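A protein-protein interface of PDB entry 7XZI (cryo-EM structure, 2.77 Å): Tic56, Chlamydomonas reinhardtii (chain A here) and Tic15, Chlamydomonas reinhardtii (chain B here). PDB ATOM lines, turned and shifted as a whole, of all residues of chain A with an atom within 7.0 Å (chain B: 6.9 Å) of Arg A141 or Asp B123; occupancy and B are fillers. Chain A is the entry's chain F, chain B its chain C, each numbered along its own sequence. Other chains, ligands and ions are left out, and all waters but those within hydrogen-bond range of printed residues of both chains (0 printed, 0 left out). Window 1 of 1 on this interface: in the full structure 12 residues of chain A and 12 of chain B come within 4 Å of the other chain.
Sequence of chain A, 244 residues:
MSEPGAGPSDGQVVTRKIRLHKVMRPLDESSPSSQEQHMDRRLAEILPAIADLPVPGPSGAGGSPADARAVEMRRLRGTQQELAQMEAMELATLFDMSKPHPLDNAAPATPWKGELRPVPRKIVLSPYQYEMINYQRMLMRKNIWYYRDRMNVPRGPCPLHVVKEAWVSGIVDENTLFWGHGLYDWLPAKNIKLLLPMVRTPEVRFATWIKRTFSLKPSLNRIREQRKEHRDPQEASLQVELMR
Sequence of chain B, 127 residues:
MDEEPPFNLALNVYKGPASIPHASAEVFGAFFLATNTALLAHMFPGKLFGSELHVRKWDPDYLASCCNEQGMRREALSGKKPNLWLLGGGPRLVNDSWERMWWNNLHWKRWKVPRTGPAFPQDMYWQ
N of Gln B122 is in hydrogen-bond range of O of Arg A141, 2.9 Å away. The guanidinium group (NH2) of Arg A137 lies within salt-bridge range of the side-chain carboxylate (OD1) of Asp B123 (3.0 Å). The guanidinium group (NH2) of Arg A137 lies within hydrogen-bond range of the backbone carbonyl oxygen (O) of Met B124, at 3.4 Å. OE1 of Gln B122 lies close to O of Asn A143, 3.5 Å away.
Printed residues of chain A that touch a printed residue of chain B: Arg A137, Met A138, Arg A141, Asn A143, Leu A160 and Met A198. Hydrophobic or aromatic side chains of chain A that line the printed part of chain B: Met A138, Leu A160 and Met A198. Of the 10 printed residues of chain B, 5 touch a printed residue of chain A. Printed residues of chain B that touch a printed residue of chain A: Pro B121, Gln B122, Asp B123, Met B124 and Tyr B125. Among the printed residues, 10 pairs touch across the chains.
Of chain B, only Pro B121, Gln B122, Asp B123 and Tyr B125 come within 4 Å of Arg A141. Asp B123 touches just these residues of chain A: Arg A137, Arg A141 and Met A198. Of the printed residues of chain B, Asn A143 touches Gln B122. Of the printed residues of chain A, Met B124 touches Arg A137. Printed residues of chain B within 4 Å of Arg A137: Asp B123 and Met B124. The nearest residue of chain B that does not touch Arg A141 is Met B124 (5.2 Å). The nearest residue of chain A that does not touch Asp B123 is Met A140 (5.3 Å). The nearest printed residue of chain A that does not touch Pro B121 is Lys A142 (4.5 Å).
Among the printed residues, merely in contact across the chains: Arg A141 with Tyr B125 (3.4 Å), Met A138 with Tyr B125 (3.4 Å), Met A198 with Asp B123 (3.5 Å), Leu A160 with Gln B122 (3.5 Å), Arg A141 with Pro B121 (3.7 Å) and Arg A141 with Asp B123 (3.8 Å).
The backbone carbonyl oxygen (O) of Leu A139 lies close to the side-chain amide oxygen (OD1) of Asn A143, at 3.5 Å.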
ATOM      1  N   ILE A 133       5.372  -1.393   0.592  1.00  0.00           N
ATOM      2  CA  ILE A 133       4.073  -1.933   0.205  1.00  0.00           C
ATOM      3  C   ILE A 133       2.949  -1.079   0.777  1.00  0.00           C
ATOM      4  O   ILE A 133       1.954  -0.804   0.097  1.00  0.00           O
ATOM      5  CB  ILE A 133       3.951  -3.406   0.642  1.00  0.00           C
ATOM      6  CG1 ILE A 133       4.900  -4.289  -0.173  1.00  0.00           C
ATOM      7  CG2 ILE A 133       2.523  -3.897   0.490  1.00  0.00           C
ATOM      8  CD1 ILE A 133       4.898  -5.743   0.253  1.00  0.00           C
ATOM      9  N   GLN A 136       2.706   2.089  -1.293  1.00  0.00           N
ATOM     10  CA  GLN A 136       2.089   1.827  -2.591  1.00  0.00           C
ATOM     11  C   GLN A 136       0.588   1.601  -2.456  1.00  0.00           C
ATOM     12  O   GLN A 136      -0.193   2.057  -3.297  1.00  0.00           O
ATOM     13  CB  GLN A 136       2.755   0.628  -3.262  1.00  0.00           C
ATOM     14  CG  GLN A 136       4.201   0.863  -3.649  1.00  0.00           C
ATOM     15  CD  GLN A 136       4.725  -0.201  -4.588  1.00  0.00           C
ATOM     16  OE1 GLN A 136       4.103  -0.506  -5.605  1.00  0.00           O
ATOM     17  NE2 GLN A 136       5.872  -0.779  -4.250  1.00  0.00           N
ATOM     18  N   ARG A 137       0.167   0.885  -1.410  1.00  0.00           N
ATOM     19  CA  ARG A 137      -1.259   0.694  -1.170  1.00  0.00           C
ATOM     20  C   ARG A 137      -1.945   2.020  -0.875  1.00  0.00           C
ATOM     21  O   ARG A 137      -3.101   2.230  -1.258  1.00  0.00           O
ATOM     22  CB  ARG A 137      -1.478  -0.288  -0.021  1.00  0.00           C
ATOM     23  CG  ARG A 137      -1.043  -1.709  -0.321  1.00  0.00           C
ATOM     24  CD  ARG A 137      -1.290  -2.612   0.872  1.00  0.00           C
ATOM     25  NE  ARG A 137      -2.709  -2.729   1.179  1.00  0.00           N
ATOM     26  CZ  ARG A 137      -3.200  -3.393   2.219  1.00  0.00           C
ATOM     27  NH1 ARG A 137      -2.407  -3.999   3.087  1.00  0.00           N
ATOM     28  NH2 ARG A 137      -4.516  -3.449   2.389  1.00  0.00           N
ATOM     29  N   MET A 138      -1.252   2.921  -0.176  1.00  0.00           N
ATOM     30  CA  MET A 138      -1.796   4.253   0.060  1.00  0.00           C
ATOM     31  C   MET A 138      -1.994   5.000  -1.252  1.00  0.00           C
ATOM     32  O   MET A 138      -3.007   5.680  -1.447  1.00  0.00           O
ATOM     33  CB  MET A 138      -0.877   5.047   0.983  1.00  0.00           C
ATOM     34  CG  MET A 138      -1.464   6.376   1.422  1.00  0.00           C
ATOM     35  SD  MET A 138      -0.210   7.600   1.822  1.00  0.00           S
ATOM     36  CE  MET A 138       0.535   7.846   0.214  1.00  0.00           C
ATOM     37  N   LEU A 139      -1.024   4.891  -2.162  1.00  0.00           N
ATOM     38  CA  LEU A 139      -1.118   5.629  -3.419  1.00  0.00           C
ATOM     39  C   LEU A 139      -2.264   5.121  -4.290  1.00  0.00           C
ATOM     40  O   LEU A 139      -2.907   5.904  -4.997  1.00  0.00           O
ATOM     41  CB  LEU A 139       0.206   5.547  -4.178  1.00  0.00           C
ATOM     42  CG  LEU A 139       1.322   6.456  -3.667  1.00  0.00           C
ATOM     43  CD1 LEU A 139       2.535   6.371  -4.573  1.00  0.00           C
ATOM     44  CD2 LEU A 139       0.824   7.888  -3.567  1.00  0.00           C
ATOM     45  N   MET A 140      -2.534   3.817  -4.256  1.00  0.00           N
ATOM     46  CA  MET A 140      -3.485   3.202  -5.172  1.00  0.00           C
ATOM     47  C   MET A 140      -4.832   2.876  -4.534  1.00  0.00           C
ATOM     48  O   MET A 140      -5.608   2.117  -5.123  1.00  0.00           O
ATOM     49  CB  MET A 140      -2.882   1.927  -5.772  1.00  0.00           C
ATOM     50  CG  MET A 140      -1.592   2.156  -6.539  1.00  0.00           C
ATOM     51  SD  MET A 140      -0.986   0.654  -7.329  1.00  0.00           S
ATOM     52  CE  MET A 140      -0.862  -0.438  -5.917  1.00  0.00           C
ATOM     53  N   ARG A 141      -5.133   3.422  -3.355  1.00  0.00           N
ATOM     54  CA  ARG A 141      -6.360   3.030  -2.667  1.00  0.00           C
ATOM     55  C   ARG A 141      -7.599   3.670  -3.286  1.00  0.00           C
ATOM     56  O   ARG A 141      -8.723   3.256  -2.982  1.00  0.00           O
ATOM     57  CB  ARG A 141      -6.269   3.373  -1.181  1.00  0.00           C
ATOM     58  CG  ARG A 141      -6.134   4.853  -0.872  1.00  0.00           C
ATOM     59  CD  ARG A 141      -6.072   5.071   0.629  1.00  0.00           C
ATOM     60  NE  ARG A 141      -5.938   6.475   0.983  1.00  0.00           N
ATOM     61  CZ  ARG A 141      -5.864   6.929   2.229  1.00  0.00           C
ATOM     62  NH1 ARG A 141      -5.909   6.109   3.265  1.00  0.00           N
ATOM     63  NH2 ARG A 141      -5.739   8.235   2.436  1.00  0.00           N
ATOM     64  N   LYS A 142      -7.423   4.676  -4.144  1.00  0.00           N
ATOM     65  CA  LYS A 142      -8.543   5.352  -4.791  1.00  0.00           C
ATOM     66  C   LYS A 142      -8.514   5.212  -6.311  1.00  0.00           C
ATOM     67  O   LYS A 142      -9.146   6.007  -7.012  1.00  0.00           O
ATOM     68  CB  LYS A 142      -8.571   6.831  -4.404  1.00  0.00           C
ATOM     69  CG  LYS A 142      -8.701   7.091  -2.914  1.00  0.00           C
ATOM     70  CD  LYS A 142      -8.927   8.570  -2.639  1.00  0.00           C
ATOM     71  CE  LYS A 142      -8.914   8.870  -1.149  1.00  0.00           C
ATOM     72  NZ  LYS A 142      -7.577   8.618  -0.545  1.00  0.00           N
ATOM     73  N   ASN A 143      -7.792   4.225  -6.833  1.00  0.00           N
ATOM     74  CA  ASN A 143      -7.619   4.115  -8.273  1.00  0.00           C
ATOM     75  C   ASN A 143      -8.867   3.554  -8.947  1.00  0.00           C
ATOM     76  O   ASN A 143      -9.636   2.793  -8.356  1.00  0.00           O
ATOM     77  CB  ASN A 143      -6.414   3.234  -8.601  1.00  0.00           C
ATOM     78  CG  ASN A 143      -5.095   3.919  -8.308  1.00  0.00           C
ATOM     79  OD1 ASN A 143      -5.040   4.895  -7.560  1.00  0.00           O
ATOM     80  ND2 ASN A 143      -4.020   3.410  -8.899  1.00  0.00           N
ATOM     81  N   LEU A 160     -12.665  -1.585  -7.977  1.00  0.00           N
ATOM     82  CA  LEU A 160     -12.059  -2.842  -7.541  1.00  0.00           C
ATOM     83  C   LEU A 160     -13.053  -3.998  -7.589  1.00  0.00           C
ATOM     84  O   LEU A 160     -12.708  -5.102  -8.027  1.00  0.00           O
ATOM     85  CB  LEU A 160     -11.487  -2.686  -6.134  1.00  0.00           C
ATOM     86  CG  LEU A 160     -10.644  -3.854  -5.624  1.00  0.00           C
ATOM     87  CD1 LEU A 160      -9.518  -4.150  -6.599  1.00  0.00           C
ATOM     88  CD2 LEU A 160     -10.091  -3.558  -4.240  1.00  0.00           C
ATOM     89  N   LEU A 194       0.763  -4.178  -7.632  1.00  0.00           N
ATOM     90  CA  LEU A 194      -0.217  -4.730  -6.696  1.00  0.00           C
ATOM     91  C   LEU A 194      -1.600  -4.630  -7.328  1.00  0.00           C
ATOM     92  O   LEU A 194      -2.346  -3.684  -7.060  1.00  0.00           O
ATOM     93  CB  LEU A 194      -0.165  -3.997  -5.360  1.00  0.00           C
ATOM     94  CG  LEU A 194       1.187  -3.949  -4.655  1.00  0.00           C
ATOM     95  CD1 LEU A 194       1.094  -3.120  -3.386  1.00  0.00           C
ATOM     96  CD2 LEU A 194       1.663  -5.354  -4.345  1.00  0.00           C
ATOM     97  N   MET A 198      -4.931  -7.632  -4.771  1.00  0.00           N
ATOM     98  CA  MET A 198      -6.196  -6.967  -4.473  1.00  0.00           C
ATOM     99  C   MET A 198      -7.387  -7.787  -4.955  1.00  0.00           C
ATOM    100  O   MET A 198      -8.378  -7.934  -4.231  1.00  0.00           O
ATOM    101  CB  MET A 198      -6.223  -5.577  -5.107  1.00  0.00           C
ATOM    102  CG  MET A 198      -5.185  -4.617  -4.555  1.00  0.00           C
ATOM    103  SD  MET A 198      -5.297  -2.973  -5.287  1.00  0.00           S
ATOM    104  CE  MET A 198      -4.035  -2.107  -4.358  1.00  0.00           C
ATOM    105  N   HIS B  42     -16.814  -2.241   5.785  1.00  0.00           N
ATOM    106  CA  HIS B  42     -16.402  -1.423   4.650  1.00  0.00           C
ATOM    107  C   HIS B  42     -14.898  -1.182   4.649  1.00  0.00           C
ATOM    108  O   HIS B  42     -14.287  -1.115   3.578  1.00  0.00           O
ATOM    109  CB  HIS B  42     -17.153  -0.092   4.659  1.00  0.00           C
ATOM    110  CG  HIS B  42     -18.548  -0.180   4.121  1.00  0.00           C
ATOM    111  ND1 HIS B  42     -18.941  -1.155   3.229  1.00  0.00           N
ATOM    112  CD2 HIS B  42     -19.641   0.584   4.348  1.00  0.00           C
ATOM    113  CE1 HIS B  42     -20.216  -0.985   2.929  1.00  0.00           C
ATOM    114  NE2 HIS B  42     -20.664   0.063   3.595  1.00  0.00           N
ATOM    115  N   MET B  43     -14.287  -1.047   5.830  1.00  0.00           N
ATOM    116  CA  MET B  43     -12.848  -0.796   5.886  1.00  0.00           C
ATOM    117  C   MET B  43     -12.044  -1.974   5.345  1.00  0.00           C
ATOM    118  O   MET B  43     -11.064  -1.778   4.619  1.00  0.00           O
ATOM    119  CB  MET B  43     -12.421  -0.473   7.317  1.00  0.00           C
ATOM    120  CG  MET B  43     -12.886   0.882   7.813  1.00  0.00           C
ATOM    121  SD  MET B  43     -12.092   1.366   9.356  1.00  0.00           S
ATOM    122  CE  MET B  43     -10.378   1.425   8.846  1.00  0.00           C
ATOM    123  N   PRO B  45     -12.293  -5.172   3.057  1.00  0.00           N
ATOM    124  CA  PRO B  45     -13.134  -5.938   2.120  1.00  0.00           C
ATOM    125  C   PRO B  45     -12.986  -7.446   2.245  1.00  0.00           C
ATOM    126  O   PRO B  45     -13.979  -8.169   2.115  1.00  0.00           O
ATOM    127  CB  PRO B  45     -12.667  -5.437   0.743  1.00  0.00           C
ATOM    128  CG  PRO B  45     -11.942  -4.152   1.013  1.00  0.00           C
ATOM    129  CD  PRO B  45     -11.315  -4.326   2.356  1.00  0.00           C
ATOM    130  N   PHE B 120     -15.564   5.899   0.096  1.00  0.00           N
ATOM    131  CA  PHE B 120     -14.428   5.598   0.948  1.00  0.00           C
ATOM    132  C   PHE B 120     -13.317   4.930   0.140  1.00  0.00           C
ATOM    133  O   PHE B 120     -13.567   4.361  -0.925  1.00  0.00           O
ATOM    134  CB  PHE B 120     -14.857   4.701   2.107  1.00  0.00           C
ATOM    135  CG  PHE B 120     -15.726   3.547   1.696  1.00  0.00           C
ATOM    136  CD1 PHE B 120     -15.164   2.358   1.260  1.00  0.00           C
ATOM    137  CD2 PHE B 120     -17.105   3.647   1.757  1.00  0.00           C
ATOM    138  CE1 PHE B 120     -15.963   1.296   0.886  1.00  0.00           C
ATOM    139  CE2 PHE B 120     -17.908   2.590   1.383  1.00  0.00           C
ATOM    140  CZ  PHE B 120     -17.337   1.412   0.948  1.00  0.00           C
ATOM    141  N   PRO B 121     -12.073   5.007   0.616  1.00  0.00           N
ATOM    142  CA  PRO B 121     -10.975   4.323  -0.082  1.00  0.00           C
ATOM    143  C   PRO B 121     -11.213   2.821  -0.154  1.00  0.00           C
ATOM    144  O   PRO B 121     -11.702   2.203   0.794  1.00  0.00           O
ATOM    145  CB  PRO B 121      -9.745   4.666   0.768  1.00  0.00           C
ATOM    146  CG  PRO B 121     -10.289   5.101   2.090  1.00  0.00           C
ATOM    147  CD  PRO B 121     -11.590   5.765   1.783  1.00  0.00           C
ATOM    148  N   GLN B 122     -10.850   2.236  -1.298  1.00  0.00           N
ATOM    149  CA  GLN B 122     -11.146   0.829  -1.545  1.00  0.00           C
ATOM    150  C   GLN B 122     -10.215  -0.089  -0.761  1.00  0.00           C
ATOM    151  O   GLN B 122     -10.644  -1.139  -0.268  1.00  0.00           O
ATOM    152  CB  GLN B 122     -11.053   0.540  -3.042  1.00  0.00           C
ATOM    153  CG  GLN B 122     -12.004   1.379  -3.881  1.00  0.00           C
ATOM    154  CD  GLN B 122     -11.676   1.339  -5.360  1.00  0.00           C
ATOM    155  OE1 GLN B 122     -10.699   0.718  -5.778  1.00  0.00           O
ATOM    156  NE2 GLN B 122     -12.494   2.010  -6.163  1.00  0.00           N
ATOM    157  N   ASP B 123      -8.946   0.280  -0.636  1.00  0.00           N
ATOM    158  CA  ASP B 123      -7.966  -0.542   0.050  1.00  0.00           C
ATOM    159  C   ASP B 123      -7.728   0.008   1.457  1.00  0.00           C
ATOM    160  O   ASP B 123      -8.391   0.948   1.903  1.00  0.00           O
ATOM    161  CB  ASP B 123      -6.675  -0.614  -0.768  1.00  0.00           C
ATOM    162  CG  ASP B 123      -5.897  -1.889  -0.512  1.00  0.00           C
ATOM    163  OD1 ASP B 123      -6.439  -2.788   0.164  1.00  0.00           O
ATOM    164  OD2 ASP B 123      -4.745  -1.993  -0.981  1.00  0.00           O
ATOM    165  N   MET B 124      -6.770  -0.581   2.168  1.00  0.00           N
ATOM    166  CA  MET B 124      -6.480  -0.222   3.548  1.00  0.00           C
ATOM    167  C   MET B 124      -5.081   0.368   3.647  1.00  0.00           C
ATOM    168  O   MET B 124      -4.124  -0.192   3.102  1.00  0.00           O
ATOM    169  CB  MET B 124      -6.607  -1.432   4.475  1.00  0.00           C
ATOM    170  CG  MET B 124      -6.326  -1.119   5.935  1.00  0.00           C
ATOM    171  SD  MET B 124      -7.398   0.178   6.584  1.00  0.00           S
ATOM    172  CE  MET B 124      -6.783   0.321   8.259  1.00  0.00           C
ATOM    173  N   TYR B 125      -4.969   1.494   4.345  1.00  0.00           N
ATOM    174  CA  TYR B 125      -3.707   2.177   4.574  1.00  0.00           C
ATOM    175  C   TYR B 125      -3.399   2.184   6.066  1.00  0.00           C
ATOM    176  O   TYR B 125      -4.306   2.082   6.899  1.00  0.00           O
ATOM    177  CB  TYR B 125      -3.747   3.611   4.022  1.00  0.00           C
ATOM    178  CG  TYR B 125      -2.683   4.529   4.575  1.00  0.00           C
ATOM    179  CD1 TYR B 125      -1.344   4.335   4.267  1.00  0.00           C
ATOM    180  CD2 TYR B 125      -3.016   5.590   5.403  1.00  0.00           C
ATOM    181  CE1 TYR B 125      -0.368   5.169   4.771  1.00  0.00           C
ATOM    182  CE2 TYR B 125      -2.047   6.431   5.912  1.00  0.00           C
ATOM    183  CZ  TYR B 125      -0.725   6.215   5.591  1.00  0.00           C
ATOM    184  OH  TYR B 125       0.245   7.049   6.096  1.00  0.00           O
ATOM    185  N   TRP B 126      -2.103   2.253   6.386  1.00  0.00           N
ATOM    186  CA  TRP B 126      -1.588   2.314   7.753  1.00  0.00           C
ATOM    187  C   TRP B 126      -1.702   0.960   8.442  1.00  0.00           C
ATOM    188  O   TRP B 126      -1.247   0.796   9.577  1.00  0.00           O
ATOM    189  CB  TRP B 126      -2.307   3.394   8.568  1.00  0.00           C
ATOM    190  CG  TRP B 126      -1.421   4.513   9.000  1.00  0.00           C
ATOM    191  CD1 TRP B 126      -0.058   4.518   9.022  1.00  0.00           C
ATOM    192  CD2 TRP B 126      -1.835   5.802   9.468  1.00  0.00           C
ATOM    193  NE1 TRP B 126       0.404   5.729   9.478  1.00  0.00           N
ATOM    194  CE2 TRP B 126      -0.667   6.534   9.759  1.00  0.00           C
ATOM    195  CE3 TRP B 126      -3.079   6.408   9.671  1.00  0.00           C
ATOM    196  CZ2 TRP B 126      -0.706   7.841  10.240  1.00  0.00           C
ATOM    197  CZ3 TRP B 126      -3.116   7.702  10.149  1.00  0.00           C
ATOM    198  CH2 TRP B 126      -1.937   8.405  10.428  1.00  0.00           C
